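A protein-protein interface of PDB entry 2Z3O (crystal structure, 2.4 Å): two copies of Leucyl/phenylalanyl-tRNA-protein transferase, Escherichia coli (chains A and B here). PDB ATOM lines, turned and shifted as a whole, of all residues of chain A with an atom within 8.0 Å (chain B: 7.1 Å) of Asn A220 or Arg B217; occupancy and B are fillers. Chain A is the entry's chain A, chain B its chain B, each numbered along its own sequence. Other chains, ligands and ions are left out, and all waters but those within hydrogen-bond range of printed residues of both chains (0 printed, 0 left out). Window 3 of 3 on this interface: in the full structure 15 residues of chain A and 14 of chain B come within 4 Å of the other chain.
Printed residues of chain A that touch a printed residue of chain B: Leu A125, Asn A220, Asn A221 and Val A224.
Hydrophobic or aromatic side chains of chain A that line the printed part of chain B: Val A224.
Hydrophobic or aromatic side chains of chain B that line the printed part of chain A: Leu B215.
Among the printed residues, no Asp or Glu carboxylate lies within 4 Å of a Lys or Arg side-chain nitrogen of the other chain.
The guanidinium group (NH2) of Arg B217 lies within hydrogen-bond range of the side-chain amide oxygen (OD1) of Asn B220.
NH1 of Arg B217 sits at hydrogen-bond distance from OD1 of Asn A220 (2.8 Å).
The side-chain amide nitrogen (ND2) of Asn A221 sits at hydrogen-bond distance from the backbone carbonyl oxygen (O) of Leu B215 (3.1 Å).
Asn A220 touches Arg B217, but with the chains exchanged Arg A217 does not touch Asn B220 (6.7 Å).
Of the 6 pairs that touch across the chains among the printed residues, none has its exchanged pair printed and touching as well.
Of the printed residues of chain B, Leu A125 touches Asn B220 (3.3 Å).
Asn A220 touches one residue of chain B.
Of the printed residues of chain B, Asn A221 touches Leu B215 (3.1 Å).
Of the printed residues of chain B, Val A224 touches Leu B215, Gly B216 and Arg B217.
Of the printed residues of chain A, Leu B215 touches Asn A221 and Val A224.
Of chain A, only Asn A220 (2.8 Å) and Val A224 (3.7 Å) come within 4 Å of Arg B217.
Of the printed residues of chain A, Asn B220 touches Leu A125 (3.3 Å).
The nearest residue of chain B that does not touch Asn A220 is Leu B215 (6.5 Å).
The nearest residue of chain A that does not touch Arg B217 is Asn A221 (4.2 Å).
Leu A125 touches Asn B220.
Leu B215 touches Val A224.
Val A224 touches Gly B216.
CG1 of Val A224 touches CB of Arg B217, 3.7 Å away.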
ATOM      1  N   LEU A 125       8.405   1.085  23.568  1.00  0.00           N
ATOM      2  CA  LEU A 125       8.528   2.502  23.870  1.00  0.00           C
ATOM      3  C   LEU A 125       9.834   2.894  24.550  1.00  0.00           C
ATOM      4  O   LEU A 125      10.072   4.083  24.789  1.00  0.00           O
ATOM      5  CB  LEU A 125       7.350   2.944  24.735  1.00  0.00           C
ATOM      6  CG  LEU A 125       6.021   2.811  23.996  1.00  0.00           C
ATOM      7  CD1 LEU A 125       4.853   3.040  24.934  1.00  0.00           C
ATOM      8  CD2 LEU A 125       6.014   3.806  22.847  1.00  0.00           C
ATOM      9  N   GLY A 126      10.664   1.904  24.881  1.00  0.00           N
ATOM     10  CA  GLY A 126      11.948   2.186  25.512  1.00  0.00           C
ATOM     11  C   GLY A 126      12.002   2.323  27.031  1.00  0.00           C
ATOM     12  O   GLY A 126      12.891   2.987  27.560  1.00  0.00           O
ATOM     13  N   HIS A 179      27.946   2.919  34.677  1.00  0.00           N
ATOM     14  CA  HIS A 179      27.389   4.138  34.110  1.00  0.00           C
ATOM     15  C   HIS A 179      26.396   4.924  34.950  1.00  0.00           C
ATOM     16  O   HIS A 179      25.538   5.606  34.398  1.00  0.00           O
ATOM     17  CB  HIS A 179      26.762   3.842  32.750  1.00  0.00           C
ATOM     18  CG  HIS A 179      27.727   3.301  31.743  1.00  0.00           C
ATOM     19  ND1 HIS A 179      28.223   2.017  31.803  1.00  0.00           N
ATOM     20  CD2 HIS A 179      28.271   3.862  30.637  1.00  0.00           C
ATOM     21  CE1 HIS A 179      29.026   1.808  30.775  1.00  0.00           C
ATOM     22  NE2 HIS A 179      29.072   2.913  30.053  1.00  0.00           N
ATOM     23  N   ARG A 217      19.784   9.939  35.530  1.00  0.00           N
ATOM     24  CA  ARG A 217      19.945   9.799  34.101  1.00  0.00           C
ATOM     25  C   ARG A 217      21.168   8.941  33.789  1.00  0.00           C
ATOM     26  O   ARG A 217      22.263   9.186  34.295  1.00  0.00           O
ATOM     27  CB  ARG A 217      20.096  11.193  33.478  1.00  0.00           C
ATOM     28  CG  ARG A 217      20.108  11.214  31.968  1.00  0.00           C
ATOM     29  CD  ARG A 217      18.749  11.594  31.393  1.00  0.00           C
ATOM     30  NE  ARG A 217      18.534  10.966  30.085  1.00  0.00           N
ATOM     31  CZ  ARG A 217      17.548  11.276  29.244  1.00  0.00           C
ATOM     32  NH1 ARG A 217      16.672  12.223  29.563  1.00  0.00           N
ATOM     33  NH2 ARG A 217      17.427  10.620  28.092  1.00  0.00           N
ATOM     34  N   LEU A 218      20.967   7.914  32.974  1.00  0.00           N
ATOM     35  CA  LEU A 218      22.055   7.034  32.572  1.00  0.00           C
ATOM     36  C   LEU A 218      22.539   7.572  31.239  1.00  0.00           C
ATOM     37  O   LEU A 218      21.914   8.453  30.675  1.00  0.00           O
ATOM     38  CB  LEU A 218      21.546   5.604  32.398  1.00  0.00           C
ATOM     39  CG  LEU A 218      21.228   4.846  33.682  1.00  0.00           C
ATOM     40  CD1 LEU A 218      20.768   3.442  33.335  1.00  0.00           C
ATOM     41  CD2 LEU A 218      22.475   4.791  34.563  1.00  0.00           C
ATOM     42  N   PRO A 219      23.669   7.066  30.728  1.00  0.00           N
ATOM     43  CA  PRO A 219      24.150   7.566  29.441  1.00  0.00           C
ATOM     44  C   PRO A 219      23.020   7.489  28.433  1.00  0.00           C
ATOM     45  O   PRO A 219      22.167   6.605  28.509  1.00  0.00           O
ATOM     46  CB  PRO A 219      25.295   6.621  29.113  1.00  0.00           C
ATOM     47  CG  PRO A 219      25.875   6.352  30.462  1.00  0.00           C
ATOM     48  CD  PRO A 219      24.631   6.110  31.309  1.00  0.00           C
ATOM     49  N   ASN A 220      23.020   8.416  27.488  1.00  0.00           N
ATOM     50  CA  ASN A 220      21.981   8.480  26.478  1.00  0.00           C
ATOM     51  C   ASN A 220      21.744   7.211  25.664  1.00  0.00           C
ATOM     52  O   ASN A 220      20.644   6.996  25.162  1.00  0.00           O
ATOM     53  CB  ASN A 220      22.264   9.631  25.516  1.00  0.00           C
ATOM     54  CG  ASN A 220      21.003  10.351  25.109  1.00  0.00           C
ATOM     55  OD1 ASN A 220      20.060   9.734  24.604  1.00  0.00           O
ATOM     56  ND2 ASN A 220      20.968  11.666  25.338  1.00  0.00           N
ATOM     57  N   ASN A 221      22.763   6.371  25.533  1.00  0.00           N
ATOM     58  CA  ASN A 221      22.616   5.156  24.748  1.00  0.00           C
ATOM     59  C   ASN A 221      22.770   3.887  25.576  1.00  0.00           C
ATOM     60  O   ASN A 221      22.911   2.798  25.020  1.00  0.00           O
ATOM     61  CB  ASN A 221      23.648   5.162  23.629  1.00  0.00           C
ATOM     62  CG  ASN A 221      25.060   5.174  24.158  1.00  0.00           C
ATOM     63  OD1 ASN A 221      25.314   5.671  25.260  1.00  0.00           O
ATOM     64  ND2 ASN A 221      25.994   4.635  23.378  1.00  0.00           N
ATOM     65  N   PHE A 222      22.723   4.028  26.896  1.00  0.00           N
ATOM     66  CA  PHE A 222      22.883   2.886  27.796  1.00  0.00           C
ATOM     67  C   PHE A 222      22.081   1.651  27.410  1.00  0.00           C
ATOM     68  O   PHE A 222      22.594   0.539  27.458  1.00  0.00           O
ATOM     69  CB  PHE A 222      22.512   3.268  29.234  1.00  0.00           C
ATOM     70  CG  PHE A 222      22.783   2.175  30.234  1.00  0.00           C
ATOM     71  CD1 PHE A 222      24.083   1.920  30.671  1.00  0.00           C
ATOM     72  CD2 PHE A 222      21.752   1.355  30.688  1.00  0.00           C
ATOM     73  CE1 PHE A 222      24.353   0.864  31.538  1.00  0.00           C
ATOM     74  CE2 PHE A 222      22.008   0.295  31.554  1.00  0.00           C
ATOM     75  CZ  PHE A 222      23.317   0.048  31.981  1.00  0.00           C
ATOM     76  N   TRP A 223      20.832   1.864  27.010  1.00  0.00           N
ATOM     77  CA  TRP A 223      19.929   0.781  26.665  1.00  0.00           C
ATOM     78  C   TRP A 223      19.840   0.323  25.205  1.00  0.00           C
ATOM     79  O   TRP A 223      19.069  -0.580  24.896  1.00  0.00           O
ATOM     80  CB  TRP A 223      18.519   1.122  27.156  1.00  0.00           C
ATOM     81  CG  TRP A 223      18.411   1.417  28.635  1.00  0.00           C
ATOM     82  CD1 TRP A 223      18.275   2.643  29.218  1.00  0.00           C
ATOM     83  CD2 TRP A 223      18.445   0.465  29.715  1.00  0.00           C
ATOM     84  NE1 TRP A 223      18.223   2.517  30.590  1.00  0.00           N
ATOM     85  CE2 TRP A 223      18.326   1.193  30.919  1.00  0.00           C
ATOM     86  CE3 TRP A 223      18.569  -0.928  29.779  1.00  0.00           C
ATOM     87  CZ2 TRP A 223      18.326   0.578  32.166  1.00  0.00           C
ATOM     88  CZ3 TRP A 223      18.568  -1.542  31.020  1.00  0.00           C
ATOM     89  CH2 TRP A 223      18.447  -0.788  32.199  1.00  0.00           C
ATOM     90  N   VAL A 224      20.596   0.918  24.296  1.00  0.00           N
ATOM     91  CA  VAL A 224      20.497   0.463  22.910  1.00  0.00           C
ATOM     92  C   VAL A 224      21.024  -0.968  22.854  1.00  0.00           C
ATOM     93  O   VAL A 224      21.861  -1.357  23.653  1.00  0.00           O
ATOM     94  CB  VAL A 224      21.323   1.336  21.923  1.00  0.00           C
ATOM     95  CG1 VAL A 224      21.014   2.802  22.133  1.00  0.00           C
ATOM     96  CG2 VAL A 224      22.795   1.065  22.089  1.00  0.00           C
ATOM     97  N   PRO A 225      20.529  -1.763  21.906  1.00  0.00           N
ATOM     98  CA  PRO A 225      20.943  -3.161  21.733  1.00  0.00           C
ATOM     99  C   PRO A 225      22.432  -3.316  21.527  1.00  0.00           C
ATOM    100  O   PRO A 225      23.019  -2.636  20.690  1.00  0.00           O
ATOM    101  CB  PRO A 225      20.141  -3.612  20.514  1.00  0.00           C
ATOM    102  CG  PRO A 225      19.911  -2.310  19.761  1.00  0.00           C
ATOM    103  CD  PRO A 225      19.557  -1.369  20.874  1.00  0.00           C
ATOM    104  N   GLY B 149      21.388   0.753  15.000  1.00  0.00           N
ATOM    105  CA  GLY B 149      21.571   2.086  15.530  1.00  0.00           C
ATOM    106  C   GLY B 149      21.062   3.072  14.504  1.00  0.00           C
ATOM    107  O   GLY B 149      20.004   2.876  13.919  1.00  0.00           O
ATOM    108  N   THR B 150      21.828   4.130  14.279  1.00  0.00           N
ATOM    109  CA  THR B 150      21.487   5.175  13.325  1.00  0.00           C
ATOM    110  C   THR B 150      21.771   4.702  11.899  1.00  0.00           C
ATOM    111  O   THR B 150      21.655   5.475  10.947  1.00  0.00           O
ATOM    112  CB  THR B 150      22.331   6.428  13.598  1.00  0.00           C
ATOM    113  OG1 THR B 150      23.717   6.106  13.419  1.00  0.00           O
ATOM    114  CG2 THR B 150      22.140   6.906  15.021  1.00  0.00           C
ATOM    115  N   HIS B 179      15.305  12.406  11.995  1.00  0.00           N
ATOM    116  CA  HIS B 179      15.409  11.956  13.372  1.00  0.00           C
ATOM    117  C   HIS B 179      16.743  11.348  13.754  1.00  0.00           C
ATOM    118  O   HIS B 179      16.801  10.467  14.600  1.00  0.00           O
ATOM    119  CB  HIS B 179      14.291  10.967  13.687  1.00  0.00           C
ATOM    120  CG  HIS B 179      12.952  11.609  13.839  1.00  0.00           C
ATOM    121  ND1 HIS B 179      11.918  11.399  12.952  1.00  0.00           N
ATOM    122  CD2 HIS B 179      12.478  12.467  14.773  1.00  0.00           C
ATOM    123  CE1 HIS B 179      10.865  12.100  13.333  1.00  0.00           C
ATOM    124  NE2 HIS B 179      11.179  12.758  14.435  1.00  0.00           N
ATOM    125  N   GLY B 180      17.813  11.816  13.132  1.00  0.00           N
ATOM    126  CA  GLY B 180      19.121  11.301  13.474  1.00  0.00           C
ATOM    127  C   GLY B 180      19.650  10.235  12.550  1.00  0.00           C
ATOM    128  O   GLY B 180      20.842   9.948  12.571  1.00  0.00           O
ATOM    129  N   GLY B 181      18.777   9.640  11.743  1.00  0.00           N
ATOM    130  CA  GLY B 181      19.234   8.608  10.835  1.00  0.00           C
ATOM    131  C   GLY B 181      20.463   9.112  10.114  1.00  0.00           C
ATOM    132  O   GLY B 181      20.491  10.266   9.682  1.00  0.00           O
ATOM    133  N   MET B 213      27.893   3.804  14.296  1.00  0.00           N
ATOM    134  CA  MET B 213      26.461   4.073  14.301  1.00  0.00           C
ATOM    135  C   MET B 213      25.598   3.049  15.043  1.00  0.00           C
ATOM    136  O   MET B 213      24.471   3.359  15.421  1.00  0.00           O
ATOM    137  CB  MET B 213      25.970   4.228  12.862  1.00  0.00           C
ATOM    138  CG  MET B 213      26.515   5.464  12.173  1.00  0.00           C
ATOM    139  SD  MET B 213      26.310   5.464  10.376  1.00  0.00           S
ATOM    140  CE  MET B 213      27.997   5.653   9.849  1.00  0.00           C
ATOM    141  N   ARG B 214      26.112   1.837  15.261  1.00  0.00           N
ATOM    142  CA  ARG B 214      25.319   0.833  15.981  1.00  0.00           C
ATOM    143  C   ARG B 214      25.044   1.205  17.434  1.00  0.00           C
ATOM    144  O   ARG B 214      24.039   0.790  17.997  1.00  0.00           O
ATOM    145  CB  ARG B 214      25.973  -0.557  15.920  1.00  0.00           C
ATOM    146  CG  ARG B 214      27.455  -0.599  16.186  1.00  0.00           C
ATOM    147  CD  ARG B 214      28.022  -1.980  15.841  1.00  0.00           C
ATOM    148  NE  ARG B 214      27.838  -2.934  16.927  1.00  0.00           N
ATOM    149  CZ  ARG B 214      28.627  -3.004  17.994  1.00  0.00           C
ATOM    150  NH1 ARG B 214      29.661  -2.184  18.117  1.00  0.00           N
ATOM    151  NH2 ARG B 214      28.373  -3.883  18.947  1.00  0.00           N
ATOM    152  N   LEU B 215      25.916   2.000  18.042  1.00  0.00           N
ATOM    153  CA  LEU B 215      25.693   2.386  19.433  1.00  0.00           C
ATOM    154  C   LEU B 215      24.902   3.675  19.552  1.00  0.00           C
ATOM    155  O   LEU B 215      24.608   4.139  20.654  1.00  0.00           O
ATOM    156  CB  LEU B 215      27.019   2.496  20.180  1.00  0.00           C
ATOM    157  CG  LEU B 215      27.750   1.154  20.165  1.00  0.00           C
ATOM    158  CD1 LEU B 215      29.169   1.299  20.698  1.00  0.00           C
ATOM    159  CD2 LEU B 215      26.926   0.156  20.976  1.00  0.00           C
ATOM    160  N   GLY B 216      24.553   4.251  18.409  1.00  0.00           N
ATOM    161  CA  GLY B 216      23.755   5.460  18.420  1.00  0.00           C
ATOM    162  C   GLY B 216      22.305   5.052  18.606  1.00  0.00           C
ATOM    163  O   GLY B 216      22.000   3.881  18.844  1.00  0.00           O
ATOM    164  N   ARG B 217      21.398   6.011  18.511  1.00  0.00           N
ATOM    165  CA  ARG B 217      19.991   5.699  18.659  1.00  0.00           C
ATOM    166  C   ARG B 217      19.145   6.760  17.965  1.00  0.00           C
ATOM    167  O   ARG B 217      19.677   7.772  17.490  1.00  0.00           O
ATOM    168  CB  ARG B 217      19.631   5.604  20.143  1.00  0.00           C
ATOM    169  CG  ARG B 217      20.070   6.798  20.970  1.00  0.00           C
ATOM    170  CD  ARG B 217      19.557   6.710  22.409  1.00  0.00           C
ATOM    171  NE  ARG B 217      18.111   6.547  22.472  1.00  0.00           N
ATOM    172  CZ  ARG B 217      17.320   7.182  23.333  1.00  0.00           C
ATOM    173  NH1 ARG B 217      17.843   8.030  24.210  1.00  0.00           N
ATOM    174  NH2 ARG B 217      16.005   6.974  23.320  1.00  0.00           N
ATOM    175  N   LEU B 218      17.838   6.496  17.892  1.00  0.00           N
ATOM    176  CA  LEU B 218      16.851   7.390  17.287  1.00  0.00           C
ATOM    177  C   LEU B 218      15.757   7.536  18.346  1.00  0.00           C
ATOM    178  O   LEU B 218      15.783   6.837  19.357  1.00  0.00           O
ATOM    179  CB  LEU B 218      16.270   6.758  16.021  1.00  0.00           C
ATOM    180  CG  LEU B 218      17.247   6.338  14.923  1.00  0.00           C
ATOM    181  CD1 LEU B 218      16.490   5.633  13.814  1.00  0.00           C
ATOM    182  CD2 LEU B 218      17.978   7.562  14.377  1.00  0.00           C
ATOM    183  N   PRO B 219      14.779   8.428  18.137  1.00  0.00           N
ATOM    184  CA  PRO B 219      13.733   8.568  19.156  1.00  0.00           C
ATOM    185  C   PRO B 219      13.143   7.220  19.550  1.00  0.00           C
ATOM    186  O   PRO B 219      12.976   6.348  18.710  1.00  0.00           O
ATOM    187  CB  PRO B 219      12.707   9.463  18.474  1.00  0.00           C
ATOM    188  CG  PRO B 219      13.553  10.307  17.578  1.00  0.00           C
ATOM    189  CD  PRO B 219      14.497   9.296  16.982  1.00  0.00           C
ATOM    190  N   ASN B 220      12.827   7.063  20.830  1.00  0.00           N
ATOM    191  CA  ASN B 220      12.257   5.824  21.353  1.00  0.00           C
ATOM    192  C   ASN B 220      11.101   5.277  20.532  1.00  0.00           C
ATOM    193  O   ASN B 220      10.963   4.064  20.352  1.00  0.00           O
ATOM    194  CB  ASN B 220      11.765   6.031  22.787  1.00  0.00           C
ATOM    195  CG  ASN B 220      12.887   6.322  23.743  1.00  0.00           C
ATOM    196  OD1 ASN B 220      13.805   5.518  23.902  1.00  0.00           O
ATOM    197  ND2 ASN B 220      12.825   7.482  24.390  1.00  0.00           N
ATOM    198  N   ASN B 221      10.268   6.177  20.041  1.00  0.00           N
ATOM    199  CA  ASN B 221       9.110   5.774  19.269  1.00  0.00           C
ATOM    200  C   ASN B 221       9.343   5.745  17.767  1.00  0.00           C
ATOM    201  O   ASN B 221       8.403   5.546  17.002  1.00  0.00           O
ATOM    202  CB  ASN B 221       7.936   6.694  19.615  1.00  0.00           C
ATOM    203  CG  ASN B 221       8.329   8.169  19.621  1.00  0.00           C
ATOM    204  OD1 ASN B 221       7.656   9.004  20.235  1.00  0.00           O
ATOM    205  ND2 ASN B 221       9.415   8.495  18.930  1.00  0.00           N
